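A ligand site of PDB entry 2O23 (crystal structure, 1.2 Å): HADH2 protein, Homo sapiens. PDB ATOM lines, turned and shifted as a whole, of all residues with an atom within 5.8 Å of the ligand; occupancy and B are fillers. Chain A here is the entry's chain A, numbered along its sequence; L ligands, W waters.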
ATOM      1  N   THR A  18      -0.269 -17.184 -27.759  1.00  0.00           N
ATOM      2  CA  THR A  18      -1.443 -17.205 -28.599  1.00  0.00           C
ATOM      3  C   THR A  18      -2.342 -16.054 -28.181  1.00  0.00           C
ATOM      4  O   THR A  18      -2.396 -15.683 -26.990  1.00  0.00           O
ATOM      5  CB  THR A  18      -2.201 -18.557 -28.615  1.00  0.00           C
ATOM      6  OG1 THR A  18      -3.049 -18.627 -27.454  1.00  0.00           O
ATOM      7  CG2 THR A  18      -1.258 -19.739 -28.663  1.00  0.00           C
ATOM      8  N   GLY A  19      -3.081 -15.506 -29.132  1.00  0.00           N
ATOM      9  CA  GLY A  19      -3.801 -14.271 -28.866  1.00  0.00           C
ATOM     10  C   GLY A  19      -2.894 -13.072 -28.620  1.00  0.00           C
ATOM     11  O   GLY A  19      -3.312 -12.068 -28.036  1.00  0.00           O
ATOM     12  N   GLY A  20      -1.658 -13.143 -29.113  1.00  0.00           N
ATOM     13  CA  GLY A  20      -0.645 -12.153 -28.762  1.00  0.00           C
ATOM     14  C   GLY A  20      -0.813 -10.786 -29.414  1.00  0.00           C
ATOM     15  O   GLY A  20      -0.073  -9.860 -29.064  1.00  0.00           O
ATOM     16  N   ALA A  21      -1.760 -10.639 -30.350  1.00  0.00           N
ATOM     17  CA  ALA A  21      -1.969  -9.351 -31.021  1.00  0.00           C
ATOM     18  C   ALA A  21      -2.779  -8.360 -30.192  1.00  0.00           C
ATOM     19  O   ALA A  21      -2.829  -7.172 -30.540  1.00  0.00           O
ATOM     20  CB  ALA A  21      -2.656  -9.560 -32.371  1.00  0.00           C
ATOM     21  N   SER A  22      -3.394  -8.820 -29.093  1.00  0.00           N
ATOM     22  CA  SER A  22      -4.332  -7.976 -28.343  1.00  0.00           C
ATOM     23  C   SER A  22      -4.361  -8.329 -26.872  1.00  0.00           C
ATOM     24  O   SER A  22      -4.001  -9.427 -26.496  1.00  0.00           O
ATOM     25  CB  SER A  22      -5.736  -8.166 -28.938  1.00  0.00           C
ATOM     26  OG  SER A  22      -6.729  -7.320 -28.338  1.00  0.00           O
ATOM     27  N   GLY A  23      -4.839  -7.391 -26.047  1.00  0.00           N
ATOM     28  CA  GLY A  23      -5.307  -7.738 -24.713  1.00  0.00           C
ATOM     29  C   GLY A  23      -4.269  -8.389 -23.835  1.00  0.00           C
ATOM     30  O   GLY A  23      -3.149  -7.879 -23.717  1.00  0.00           O
ATOM     31  N   LEU A  24      -4.662  -9.475 -23.169  1.00  0.00           N
ATOM     32  CA  LEU A  24      -3.788 -10.101 -22.193  1.00  0.00           C
ATOM     33  C   LEU A  24      -2.538 -10.690 -22.850  1.00  0.00           C
ATOM     34  O   LEU A  24      -1.438 -10.653 -22.295  1.00  0.00           O
ATOM     35  CB  LEU A  24      -4.547 -11.177 -21.398  1.00  0.00           C
ATOM     36  CG  LEU A  24      -5.771 -10.707 -20.609  1.00  0.00           C
ATOM     37  CD1 LEU A  24      -6.349 -11.899 -19.784  1.00  0.00           C
ATOM     38  CD2 LEU A  24      -5.424  -9.528 -19.731  1.00  0.00           C
ATOM     39  N   GLY A  25      -2.699 -11.265 -24.051  1.00  0.00           N
ATOM     40  CA  GLY A  25      -1.573 -11.828 -24.765  1.00  0.00           C
ATOM     41  C   GLY A  25      -0.562 -10.769 -25.152  1.00  0.00           C
ATOM     42  O   GLY A  25       0.647 -10.958 -24.987  1.00  0.00           O
ATOM     43  N   LEU A  42       1.245 -15.405 -31.828  1.00  0.00           N
ATOM     44  CA  LEU A  42       0.485 -16.331 -32.635  1.00  0.00           C
ATOM     45  C   LEU A  42      -0.967 -15.872 -32.599  1.00  0.00           C
ATOM     46  O   LEU A  42      -1.583 -15.848 -31.558  1.00  0.00           O
ATOM     47  CB  LEU A  42       0.653 -17.750 -32.105  1.00  0.00           C
ATOM     48  CG  LEU A  42       0.065 -18.923 -32.904  1.00  0.00           C
ATOM     49  CD1 LEU A  42       0.675 -20.249 -32.477  1.00  0.00           C
ATOM     50  CD2 LEU A  42      -1.488 -18.956 -32.860  1.00  0.00           C
ATOM     51  N   ASP A  43      -1.458 -15.411 -33.739  1.00  0.00           N
ATOM     52  CA  ASP A  43      -2.802 -14.802 -33.771  1.00  0.00           C
ATOM     53  C   ASP A  43      -3.308 -14.858 -35.203  1.00  0.00           C
ATOM     54  O   ASP A  43      -2.575 -15.214 -36.133  1.00  0.00           O
ATOM     55  CB  ASP A  43      -2.771 -13.355 -33.214  1.00  0.00           C
ATOM     56  CG  ASP A  43      -4.088 -12.907 -32.569  1.00  0.00           C
ATOM     57  OD1 ASP A  43      -5.166 -13.102 -33.199  1.00  0.00           O
ATOM     58  OD2 ASP A  43      -4.027 -12.351 -31.440  1.00  0.00           O
ATOM     59  N   LEU A  44      -4.581 -14.554 -35.376  1.00  0.00           N
ATOM     60  CA  LEU A  44      -5.217 -14.687 -36.670  1.00  0.00           C
ATOM     61  C   LEU A  44      -4.653 -13.687 -37.704  1.00  0.00           C
ATOM     62  O   LEU A  44      -4.194 -12.615 -37.336  1.00  0.00           O
ATOM     63  CB  LEU A  44      -6.720 -14.494 -36.540  1.00  0.00           C
ATOM     64  CG  LEU A  44      -7.464 -15.588 -35.763  1.00  0.00           C
ATOM     65  CD1 LEU A  44      -8.841 -15.119 -35.386  1.00  0.00           C
ATOM     66  CD2 LEU A  44      -7.522 -16.873 -36.578  1.00  0.00           C
ATOM     67  N   SER A  47      -5.432  -9.715 -37.507  1.00  0.00           N
ATOM     68  CA  SER A  47      -5.572  -9.398 -36.083  1.00  0.00           C
ATOM     69  C   SER A  47      -4.785  -8.142 -35.654  1.00  0.00           C
ATOM     70  O   SER A  47      -4.909  -7.734 -34.497  1.00  0.00           O
ATOM     71  CB  SER A  47      -5.035 -10.546 -35.223  1.00  0.00           C
ATOM     72  OG  SER A  47      -3.658 -10.795 -35.501  1.00  0.00           O
ATOM     73  N   ALA A  65      -1.851 -17.671 -37.509  1.00  0.00           N
ATOM     74  CA  ALA A  65      -2.365 -19.025 -37.280  1.00  0.00           C
ATOM     75  C   ALA A  65      -3.684 -18.956 -36.582  1.00  0.00           C
ATOM     76  O   ALA A  65      -3.896 -18.102 -35.713  1.00  0.00           O
ATOM     77  CB  ALA A  65      -1.384 -19.845 -36.413  1.00  0.00           C
ATOM     78  N   ASP A  66      -4.555 -19.904 -36.898  1.00  0.00           N
ATOM     79  CA  ASP A  66      -5.768 -20.208 -36.138  1.00  0.00           C
ATOM     80  C   ASP A  66      -5.443 -21.372 -35.221  1.00  0.00           C
ATOM     81  O   ASP A  66      -5.019 -22.429 -35.687  1.00  0.00           O
ATOM     82  CB  ASP A  66      -6.868 -20.568 -37.151  1.00  0.00           C
ATOM     83  CG  ASP A  66      -8.237 -20.821 -36.534  1.00  0.00           C
ATOM     84  OD1 ASP A  66      -8.339 -21.201 -35.361  1.00  0.00           O
ATOM     85  OD2 ASP A  66      -9.213 -20.660 -37.298  1.00  0.00           O
ATOM     86  N   VAL A  67      -5.626 -21.185 -33.907  1.00  0.00           N
ATOM     87  CA  VAL A  67      -5.262 -22.226 -32.947  1.00  0.00           C
ATOM     88  C   VAL A  67      -6.067 -23.522 -33.128  1.00  0.00           C
ATOM     89  O   VAL A  67      -5.656 -24.561 -32.622  1.00  0.00           O
ATOM     90  CB  VAL A  67      -5.372 -21.736 -31.480  1.00  0.00           C
ATOM     91  CG1 VAL A  67      -4.327 -20.612 -31.195  1.00  0.00           C
ATOM     92  CG2 VAL A  67      -6.812 -21.312 -31.130  1.00  0.00           C
ATOM     93  N   THR A  68      -7.206 -23.479 -33.832  1.00  0.00           N
ATOM     94  CA  THR A  68      -8.006 -24.693 -34.071  1.00  0.00           C
ATOM     95  C   THR A  68      -7.464 -25.570 -35.222  1.00  0.00           C
ATOM     96  O   THR A  68      -7.937 -26.678 -35.436  1.00  0.00           O
ATOM     97  CB  THR A  68      -9.472 -24.360 -34.359  1.00  0.00           C
ATOM     98  OG1 THR A  68      -9.610 -23.644 -35.595  1.00  0.00           O
ATOM     99  CG2 THR A  68     -10.097 -23.553 -33.191  1.00  0.00           C
ATOM    100  N   ASN A  92      -1.262 -19.545 -23.577  1.00  0.00           N
ATOM    101  CA  ASN A  92      -2.525 -19.632 -24.305  1.00  0.00           C
ATOM    102  C   ASN A  92      -3.502 -18.531 -23.899  1.00  0.00           C
ATOM    103  O   ASN A  92      -4.165 -18.641 -22.873  1.00  0.00           O
ATOM    104  CB  ASN A  92      -3.162 -21.011 -24.115  1.00  0.00           C
ATOM    105  CG  ASN A  92      -2.428 -22.105 -24.829  1.00  0.00           C
ATOM    106  OD1 ASN A  92      -2.428 -22.148 -26.055  1.00  0.00           O
ATOM    107  ND2 ASN A  92      -1.806 -23.007 -24.072  1.00  0.00           N
ATOM    108  N   CYS A  93      -3.585 -17.462 -24.674  1.00  0.00           N
ATOM    109  CA  CYS A  93      -4.557 -16.376 -24.493  1.00  0.00           C
ATOM    110  C   CYS A  93      -5.629 -16.285 -25.576  1.00  0.00           C
ATOM    111  O   CYS A  93      -6.646 -15.637 -25.351  1.00  0.00           O
ATOM    112  CB  CYS A  93      -3.867 -15.014 -24.320  1.00  0.00           C
ATOM    113  SG  CYS A  93      -2.734 -14.900 -22.932  1.00  0.00           S
ATOM    114  N   ALA A  94      -5.470 -16.965 -26.703  1.00  0.00           N
ATOM    115  CA  ALA A  94      -6.487 -16.917 -27.768  1.00  0.00           C
ATOM    116  C   ALA A  94      -7.819 -17.363 -27.202  1.00  0.00           C
ATOM    117  O   ALA A  94      -7.914 -18.432 -26.581  1.00  0.00           O
ATOM    118  CB  ALA A  94      -6.077 -17.831 -28.929  1.00  0.00           C
ATOM    119  N   GLY A  95      -8.885 -16.610 -27.461  1.00  0.00           N
ATOM    120  CA  GLY A  95     -10.201 -16.990 -26.939  1.00  0.00           C
ATOM    121  C   GLY A  95     -11.276 -16.071 -27.472  1.00  0.00           C
ATOM    122  O   GLY A  95     -10.979 -14.960 -27.926  1.00  0.00           O
ATOM    123  N   ILE A  96     -12.513 -16.563 -27.376  1.00  0.00           N
ATOM    124  CA  ILE A  96     -13.717 -15.848 -27.766  1.00  0.00           C
ATOM    125  C   ILE A  96     -14.781 -16.022 -26.705  1.00  0.00           C
ATOM    126  O   ILE A  96     -14.653 -16.820 -25.790  1.00  0.00           O
ATOM    127  CB  ILE A  96     -14.252 -16.313 -29.137  1.00  0.00           C
ATOM    128  CG1 ILE A  96     -14.623 -17.793 -29.140  1.00  0.00           C
ATOM    129  CG2 ILE A  96     -13.244 -15.982 -30.264  1.00  0.00           C
ATOM    130  CD1 ILE A  96     -15.393 -18.206 -30.405  1.00  0.00           C
ATOM    131  N   VAL A 122     -12.594 -22.984 -30.159  1.00  0.00           N
ATOM    132  CA  VAL A 122     -11.506 -22.027 -30.018  1.00  0.00           C
ATOM    133  C   VAL A 122     -10.850 -22.092 -28.642  1.00  0.00           C
ATOM    134  O   VAL A 122      -9.628 -22.152 -28.518  1.00  0.00           O
ATOM    135  CB  VAL A 122     -11.951 -20.572 -30.352  1.00  0.00           C
ATOM    136  CG1 VAL A 122     -10.834 -19.587 -30.112  1.00  0.00           C
ATOM    137  CG2 VAL A 122     -12.461 -20.472 -31.810  1.00  0.00           C
ATOM    138  N   ASN A 123     -11.664 -22.032 -27.600  1.00  0.00           N
ATOM    139  CA  ASN A 123     -11.161 -21.814 -26.256  1.00  0.00           C
ATOM    140  C   ASN A 123     -10.536 -23.069 -25.680  1.00  0.00           C
ATOM    141  O   ASN A 123      -9.518 -22.987 -24.993  1.00  0.00           O
ATOM    142  CB  ASN A 123     -12.280 -21.327 -25.318  1.00  0.00           C
ATOM    143  CG  ASN A 123     -12.744 -19.929 -25.609  1.00  0.00           C
ATOM    144  OD1 ASN A 123     -12.291 -19.279 -26.545  1.00  0.00           O
ATOM    145  ND2 ASN A 123     -13.649 -19.427 -24.759  1.00  0.00           N
ATOM    146  N   THR A 155      -5.066 -19.801 -20.046  1.00  0.00           N
ATOM    147  CA  THR A 155      -5.990 -18.830 -19.509  1.00  0.00           C
ATOM    148  C   THR A 155      -7.373 -19.438 -19.422  1.00  0.00           C
ATOM    149  O   THR A 155      -7.990 -19.776 -20.431  1.00  0.00           O
ATOM    150  CB  THR A 155      -6.032 -17.539 -20.341  1.00  0.00           C
ATOM    151  OG1 THR A 155      -4.717 -17.089 -20.646  1.00  0.00           O
ATOM    152  CG2 THR A 155      -6.767 -16.423 -19.616  1.00  0.00           C
ATOM    153  N   ALA A 156      -7.856 -19.608 -18.191  1.00  0.00           N
ATOM    154  CA  ALA A 156      -9.217 -20.001 -17.911  1.00  0.00           C
ATOM    155  C   ALA A 156     -10.028 -18.715 -17.667  1.00  0.00           C
ATOM    156  O   ALA A 156      -9.965 -17.778 -18.479  1.00  0.00           O
ATOM    157  CB  ALA A 156      -9.288 -20.992 -16.804  1.00  0.00           C
ATOM    158  N   SER A 157     -10.797 -18.646 -16.575  1.00  0.00           N
ATOM    159  CA  SER A 157     -11.612 -17.489 -16.199  1.00  0.00           C
ATOM    160  C   SER A 157     -12.238 -17.862 -14.874  1.00  0.00           C
ATOM    161  O   SER A 157     -12.465 -19.060 -14.623  1.00  0.00           O
ATOM    162  CB  SER A 157     -12.745 -17.265 -17.202  1.00  0.00           C
ATOM    163  OG  SER A 157     -13.727 -16.380 -16.693  1.00  0.00           O
ATOM    164  N   VAL A 158     -12.614 -16.878 -14.061  1.00  0.00           N
ATOM    165  CA  VAL A 158     -13.424 -17.178 -12.887  1.00  0.00           C
ATOM    166  C   VAL A 158     -14.799 -17.768 -13.290  1.00  0.00           C
ATOM    167  O   VAL A 158     -15.457 -18.392 -12.464  1.00  0.00           O
ATOM    168  CB  VAL A 158     -13.585 -15.953 -11.988  1.00  0.00           C
ATOM    169  CG1 VAL A 158     -12.225 -15.514 -11.407  1.00  0.00           C
ATOM    170  CG2 VAL A 158     -14.310 -14.807 -12.695  1.00  0.00           C
ATOM    171  N   TYR A 170     -19.206 -20.444 -22.537  1.00  0.00           N
ATOM    172  CA  TYR A 170     -17.911 -19.952 -22.074  1.00  0.00           C
ATOM    173  C   TYR A 170     -17.432 -20.675 -20.826  1.00  0.00           C
ATOM    174  O   TYR A 170     -16.266 -21.089 -20.765  1.00  0.00           O
ATOM    175  CB  TYR A 170     -18.009 -18.438 -21.853  1.00  0.00           C
ATOM    176  CG  TYR A 170     -16.710 -17.732 -21.515  1.00  0.00           C
ATOM    177  CD1 TYR A 170     -15.782 -17.429 -22.503  1.00  0.00           C
ATOM    178  CD2 TYR A 170     -16.412 -17.345 -20.219  1.00  0.00           C
ATOM    179  CE1 TYR A 170     -14.565 -16.753 -22.189  1.00  0.00           C
ATOM    180  CE2 TYR A 170     -15.215 -16.708 -19.904  1.00  0.00           C
ATOM    181  CZ  TYR A 170     -14.312 -16.403 -20.890  1.00  0.00           C
ATOM    182  OH  TYR A 170     -13.152 -15.736 -20.566  1.00  0.00           O
ATOM    183  N   LYS A 174     -14.036 -22.986 -20.262  1.00  0.00           N
ATOM    184  CA  LYS A 174     -13.028 -22.619 -19.284  1.00  0.00           C
ATOM    185  C   LYS A 174     -12.925 -23.654 -18.166  1.00  0.00           C
ATOM    186  O   LYS A 174     -11.843 -23.892 -17.645  1.00  0.00           O
ATOM    187  CB  LYS A 174     -13.286 -21.203 -18.776  1.00  0.00           C
ATOM    188  CG  LYS A 174     -13.194 -20.095 -19.846  1.00  0.00           C
ATOM    189  CD  LYS A 174     -11.913 -20.134 -20.675  1.00  0.00           C
ATOM    190  CE  LYS A 174     -11.682 -18.812 -21.390  1.00  0.00           C
ATOM    191  NZ  LYS A 174     -10.271 -18.673 -21.890  1.00  0.00           N
ATOM    192  N   ALA A 199      -6.851 -17.912 -13.928  1.00  0.00           N
ATOM    193  CA  ALA A 199      -8.280 -17.638 -14.055  1.00  0.00           C
ATOM    194  C   ALA A 199      -8.545 -16.166 -13.750  1.00  0.00           C
ATOM    195  O   ALA A 199      -8.710 -15.762 -12.599  1.00  0.00           O
ATOM    196  CB  ALA A 199      -9.072 -18.545 -13.114  1.00  0.00           C
ATOM    197  N   PRO A 200      -8.512 -15.322 -14.794  1.00  0.00           N
ATOM    198  CA  PRO A 200      -8.755 -13.922 -14.560  1.00  0.00           C
ATOM    199  C   PRO A 200     -10.205 -13.609 -14.221  1.00  0.00           C
ATOM    200  O   PRO A 200     -11.133 -14.329 -14.641  1.00  0.00           O
ATOM    201  CB  PRO A 200      -8.351 -13.235 -15.889  1.00  0.00           C
ATOM    202  CG  PRO A 200      -7.628 -14.254 -16.678  1.00  0.00           C
ATOM    203  CD  PRO A 200      -8.181 -15.571 -16.216  1.00  0.00           C
ATOM    204  N   GLY A 201     -10.392 -12.483 -13.530  1.00  0.00           N
ATOM    205  CA  GLY A 201     -11.708 -11.972 -13.171  1.00  0.00           C
ATOM    206  C   GLY A 201     -12.261 -11.072 -14.266  1.00  0.00           C
ATOM    207  O   GLY A 201     -12.772 -11.565 -15.275  1.00  0.00           O
ATOM    208  N   LEU A 202     -12.172  -9.750 -14.069  1.00  0.00           N
ATOM    209  CA  LEU A 202     -12.607  -8.758 -15.060  1.00  0.00           C
ATOM    210  C   LEU A 202     -11.436  -7.848 -15.361  1.00  0.00           C
ATOM    211  O   LEU A 202     -10.936  -7.207 -14.434  1.00  0.00           O
ATOM    212  CB  LEU A 202     -13.738  -7.903 -14.524  1.00  0.00           C
ATOM    213  CG  LEU A 202     -14.999  -8.643 -14.108  1.00  0.00           C
ATOM    214  CD1 LEU A 202     -15.986  -7.714 -13.404  1.00  0.00           C
ATOM    215  CD2 LEU A 202     -15.600  -9.291 -15.342  1.00  0.00           C
ATOM    216  N   PHE A 203     -10.985  -7.831 -16.624  1.00  0.00           N
ATOM    217  CA  PHE A 203      -9.786  -7.072 -17.074  1.00  0.00           C
ATOM    218  C   PHE A 203     -10.109  -6.071 -18.182  1.00  0.00           C
ATOM    219  O   PHE A 203     -10.950  -6.316 -19.035  1.00  0.00           O
ATOM    220  CB  PHE A 203      -8.690  -8.022 -17.576  1.00  0.00           C
ATOM    221  CG  PHE A 203      -7.829  -8.505 -16.478  1.00  0.00           C
ATOM    222  CD1 PHE A 203      -8.323  -9.415 -15.561  1.00  0.00           C
ATOM    223  CD2 PHE A 203      -6.557  -8.009 -16.270  1.00  0.00           C
ATOM    224  CE1 PHE A 203      -7.570  -9.824 -14.522  1.00  0.00           C
ATOM    225  CE2 PHE A 203      -5.796  -8.434 -15.207  1.00  0.00           C
ATOM    226  CZ  PHE A 203      -6.303  -9.321 -14.337  1.00  0.00           C
ATOM    227  N   GLY A 204      -9.414  -4.940 -18.139  1.00  0.00           N
ATOM    228  CA  GLY A 204      -9.605  -3.873 -19.127  1.00  0.00           C
ATOM    229  C   GLY A 204      -8.864  -4.118 -20.433  1.00  0.00           C
ATOM    230  O   GLY A 204      -7.949  -3.377 -20.789  1.00  0.00           O
ATOM    231  N   THR A 205      -9.283  -5.151 -21.159  1.00  0.00           N
ATOM    232  CA  THR A 205      -8.831  -5.397 -22.544  1.00  0.00           C
ATOM    233  C   THR A 205      -9.979  -5.034 -23.470  1.00  0.00           C
ATOM    234  O   THR A 205     -11.043  -4.627 -22.987  1.00  0.00           O
ATOM    235  CB  THR A 205      -8.534  -6.894 -22.763  1.00  0.00           C
ATOM    236  OG1 THR A 205      -9.769  -7.598 -22.668  1.00  0.00           O
ATOM    237  CG2 THR A 205      -7.546  -7.413 -21.747  1.00  0.00           C
ATOM    238  N   PRO A 206      -9.788  -5.166 -24.799  1.00  0.00           N
ATOM    239  CA  PRO A 206     -10.933  -5.078 -25.729  1.00  0.00           C
ATOM    240  C   PRO A 206     -11.723  -6.378 -25.883  1.00  0.00           C
ATOM    241  O   PRO A 206     -11.905  -7.133 -24.923  1.00  0.00           O
ATOM    242  CB  PRO A 206     -10.284  -4.710 -27.078  1.00  0.00           C
ATOM    243  CG  PRO A 206      -8.790  -4.698 -26.845  1.00  0.00           C
ATOM    244  CD  PRO A 206      -8.523  -5.352 -25.535  1.00  0.00           C
HETATM  245  P1  LIG L   1      -8.822 -10.020 -26.789  1.00  0.00           P
HETATM  246  O1  LIG L   1     -10.053 -10.116 -27.644  1.00  0.00           O
HETATM  247  O2  LIG L   1      -8.264  -8.666 -26.539  1.00  0.00           O
HETATM  248  O3  LIG L   1      -7.651 -10.931 -27.399  1.00  0.00           O
HETATM  249  C1  LIG L   1      -7.943 -12.247 -27.834  1.00  0.00           C
HETATM  250  C2  LIG L   1      -7.035 -12.542 -29.026  1.00  0.00           C
HETATM  251  O4  LIG L   1      -7.257 -13.893 -29.403  1.00  0.00           O
HETATM  252  C3  LIG L   1      -7.298 -11.656 -30.256  1.00  0.00           C
HETATM  253  O5  LIG L   1      -6.134 -10.986 -30.735  1.00  0.00           O
HETATM  254  C4  LIG L   1      -7.865 -12.646 -31.251  1.00  0.00           C
HETATM  255  O6  LIG L   1      -7.615 -12.334 -32.607  1.00  0.00           O
HETATM  256  C5  LIG L   1      -7.254 -13.969 -30.802  1.00  0.00           C
HETATM  257  N1  LIG L   1      -7.957 -15.159 -31.302  1.00  0.00           N
HETATM  258  C6  LIG L   1      -9.326 -15.393 -31.264  1.00  0.00           C
HETATM  259  N2  LIG L   1      -9.591 -16.575 -31.863  1.00  0.00           N
HETATM  260  C7  LIG L   1      -8.381 -17.067 -32.316  1.00  0.00           C
HETATM  261  C8  LIG L   1      -8.067 -18.222 -33.013  1.00  0.00           C
HETATM  262  N3  LIG L   1      -8.952 -19.129 -33.417  1.00  0.00           N
HETATM  263  N4  LIG L   1      -6.746 -18.416 -33.288  1.00  0.00           N
HETATM  264  C9  LIG L   1      -5.785 -17.528 -32.910  1.00  0.00           C
HETATM  265  N5  LIG L   1      -6.070 -16.366 -32.265  1.00  0.00           N
HETATM  266  C10 LIG L   1      -7.374 -16.185 -31.963  1.00  0.00           C
HETATM  267  O7  LIG L   1      -9.214 -10.774 -25.427  1.00  0.00           O
HETATM  268  P2  LIG L   1      -8.492 -10.834 -23.993  1.00  0.00           P
HETATM  269  O8  LIG L   1      -9.347 -10.061 -23.044  1.00  0.00           O
HETATM  270  O9  LIG L   1      -7.045 -10.538 -24.138  1.00  0.00           O
HETATM  271  O10 LIG L   1      -8.682 -12.353 -23.671  1.00  0.00           O
HETATM  272  C11 LIG L   1      -7.570 -13.242 -23.595  1.00  0.00           C
HETATM  273  C12 LIG L   1      -7.933 -14.511 -22.831  1.00  0.00           C
HETATM  274  O11 LIG L   1      -8.337 -14.146 -21.506  1.00  0.00           O
HETATM  275  C13 LIG L   1      -9.119 -15.243 -23.448  1.00  0.00           C
HETATM  276  O12 LIG L   1      -8.969 -16.646 -23.310  1.00  0.00           O
HETATM  277  C14 LIG L   1     -10.268 -14.770 -22.565  1.00  0.00           C
HETATM  278  O13 LIG L   1     -11.339 -15.689 -22.559  1.00  0.00           O
HETATM  279  C15 LIG L   1      -9.602 -14.707 -21.221  1.00  0.00           C
HETATM  280  N6  LIG L   1     -10.254 -13.850 -20.231  1.00  0.00           N
HETATM  281  C16 LIG L   1     -10.368 -12.512 -20.424  1.00  0.00           C
HETATM  282  C17 LIG L   1     -10.968 -11.764 -19.431  1.00  0.00           C
HETATM  283  C18 LIG L   1     -11.141 -10.295 -19.574  1.00  0.00           C
HETATM  284  O14 LIG L   1     -11.897  -9.658 -18.627  1.00  0.00           O
HETATM  285  N7  LIG L   1     -10.541  -9.604 -20.516  1.00  0.00           N
HETATM  286  C19 LIG L   1     -11.428 -12.343 -18.236  1.00  0.00           C
HETATM  287  C20 LIG L   1     -11.248 -13.712 -18.063  1.00  0.00           C
HETATM  288  C21 LIG L   1     -10.651 -14.461 -19.046  1.00  0.00           C
HETATM  289  O   HOH W   1      -9.125 -11.378 -34.668  1.00  0.00           O
HETATM  290  O   HOH W   2     -14.478 -13.423 -19.548  1.00  0.00           O
HETATM  291  O   HOH W   3      -5.029 -12.060 -25.628  1.00  0.00           O
HETATM  292  O   HOH W   4     -14.591 -10.665 -19.251  1.00  0.00           O
HETATM  293  O   HOH W   5     -11.621 -12.549 -28.872  1.00  0.00           O
HETATM  294  O   HOH W   6      -7.110 -18.657 -23.955  1.00  0.00           O
HETATM  295  O   HOH W   7     -10.637  -8.633 -29.716  1.00  0.00           O
HETATM  296  O   HOH W   8      -6.891  -8.849 -32.352  1.00  0.00           O
HETATM  297  O   HOH W   9     -11.812 -17.027 -33.497  1.00  0.00           O
HETATM  298  O   HOH W  10     -13.990 -13.848 -16.155  1.00  0.00           O
HETATM  299  O   HOH W  11     -13.284 -14.243 -24.405  1.00  0.00           O
HETATM  300  O   HOH W  12     -11.303 -18.386 -35.772  1.00  0.00           O
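Water W8 bridges O5 of the ligand (2.8 Å) and O of Ser 47 (3.1 Å). Water W3 lies within hydrogen-bond range of N of Gly 25 (2.9 Å), O9 of the ligand (2.9 Å), O of Ser 22 (3.0 Å) and O of Gly 19 (3.0 Å). Water W11 bridges O13 of the ligand (3.0 Å) and O of Ile 96 (3.2 Å). Water W5 lies within hydrogen-bond range of O of Gly 95 (2.7 Å) and O1 of the ligand (3.1 Å). Water W10 lies within hydrogen-bond range of OG of Ser 157 (2.6 Å), O of Gly 201 (2.7 Å) and O of Pro 200 (3.3 Å). Water W12 lies within hydrogen-bond range of a nitrogen (N3) of the ligand and the side-chain carboxylate (OD2) of Asp 66.
O8 of the ligand sits at hydrogen-bond distance from OG1 of Thr 205 (2.5 Å). An oxygen (O5) of the ligand lies within hydrogen-bond range of the side-chain carboxylate (OD2) of Asp 43 (2.6 Å). OH of Tyr 170 is in hydrogen-bond range of O13 of the ligand (2.7 Å). An oxygen (O2) of the ligand sits at hydrogen-bond distance from the side-chain hydroxyl of Ser 22, at 2.7 Å. The backbone NH (N) of Leu 24 is in hydrogen-bond range of an oxygen (O9) of the ligand, 2.8 Å away. The side-chain amino group (NZ) of Lys 174 lies within hydrogen-bond range of an oxygen (O12) of the ligand (2.8 Å). An oxygen (O14) of the ligand sits at hydrogen-bond distance from the backbone NH (N) of Phe 203, 2.9 Å away. The side-chain carboxylate of Asp 66 sits at hydrogen-bond distance from a nitrogen (N3) of the ligand (2.9 Å). The backbone carbonyl oxygen (O) of Cys 93 lies close to an oxygen (O12) of the ligand (3.3 Å). The backbone NH (N) of Val 67 sits at hydrogen-bond distance from a nitrogen (N4) of the ligand (3.1 Å).
The backbone carbonyl oxygen (O) of Asp 43 sits at hydrogen-bond distance from the backbone NH (N) of Ala 65, 2.9 Å away. The side-chain carboxylate of Asp 43 lies within hydrogen-bond range of the backbone NH of Ala 21. OD2 of Asp 43 is in hydrogen-bond range of N of Gly 20, 3.4 Å away. The side-chain amino group (NZ) of Lys 174 sits at hydrogen-bond distance from the backbone carbonyl oxygen (O) of Thr 155, at 2.9 Å. The side-chain hydroxyl (OG1) of Thr 68 lies within hydrogen-bond range of the side-chain carboxylate (OD1) of Asp 66 (2.8 Å). N of Gly 19 sits at hydrogen-bond distance from O of Leu 42 (2.9 Å). The side-chain hydroxyl (OG1) of Thr 18 is in hydrogen-bond range of the backbone NH (N) of Ala 94 (3.0 Å). The side-chain hydroxyl (OG) of Ser 47 sits at hydrogen-bond distance from the backbone carbonyl oxygen (O) of Leu 44, at 2.6 Å.
Residues that only touch the ligand: Gly 201 (3.3 Å), Gly 23 (3.3 Å), Thr 155 (3.3 Å), Ala 65 (3.4 Å), Ala 156 (3.4 Å), Pro 206 (3.5 Å), Pro 200 (3.5 Å), Gly 19 (3.5 Å), Ala 94 (3.5 Å), Leu 44 (3.7 Å), Val 122 (3.7 Å), Gly 95 (3.7 Å), Leu 202 (3.7 Å) and Ser 157 (3.9 Å). Hydrophobic or aromatic side chains that line the ligand: Leu 24, Leu 44, Val 67, Ala 94, Val 122, Tyr 170, Pro 200, Phe 203 and Pro 206. 24 residues have an atom within 4 Å of the ligand: Gly 19, Ser 22, Gly 23, Leu 24, Asp 43, Leu 44, Ala 65, Asp 66, Val 67, Cys 93, Ala 94, Gly 95, Val 122, Thr 155, Ala 156, Ser 157, Tyr 170, Lys 174, Pro 200, Gly 201, Leu 202, Phe 203, Thr 205 and Pro 206. Along chain A the residues within 4 Å of the ligand span positions 19 to 206.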
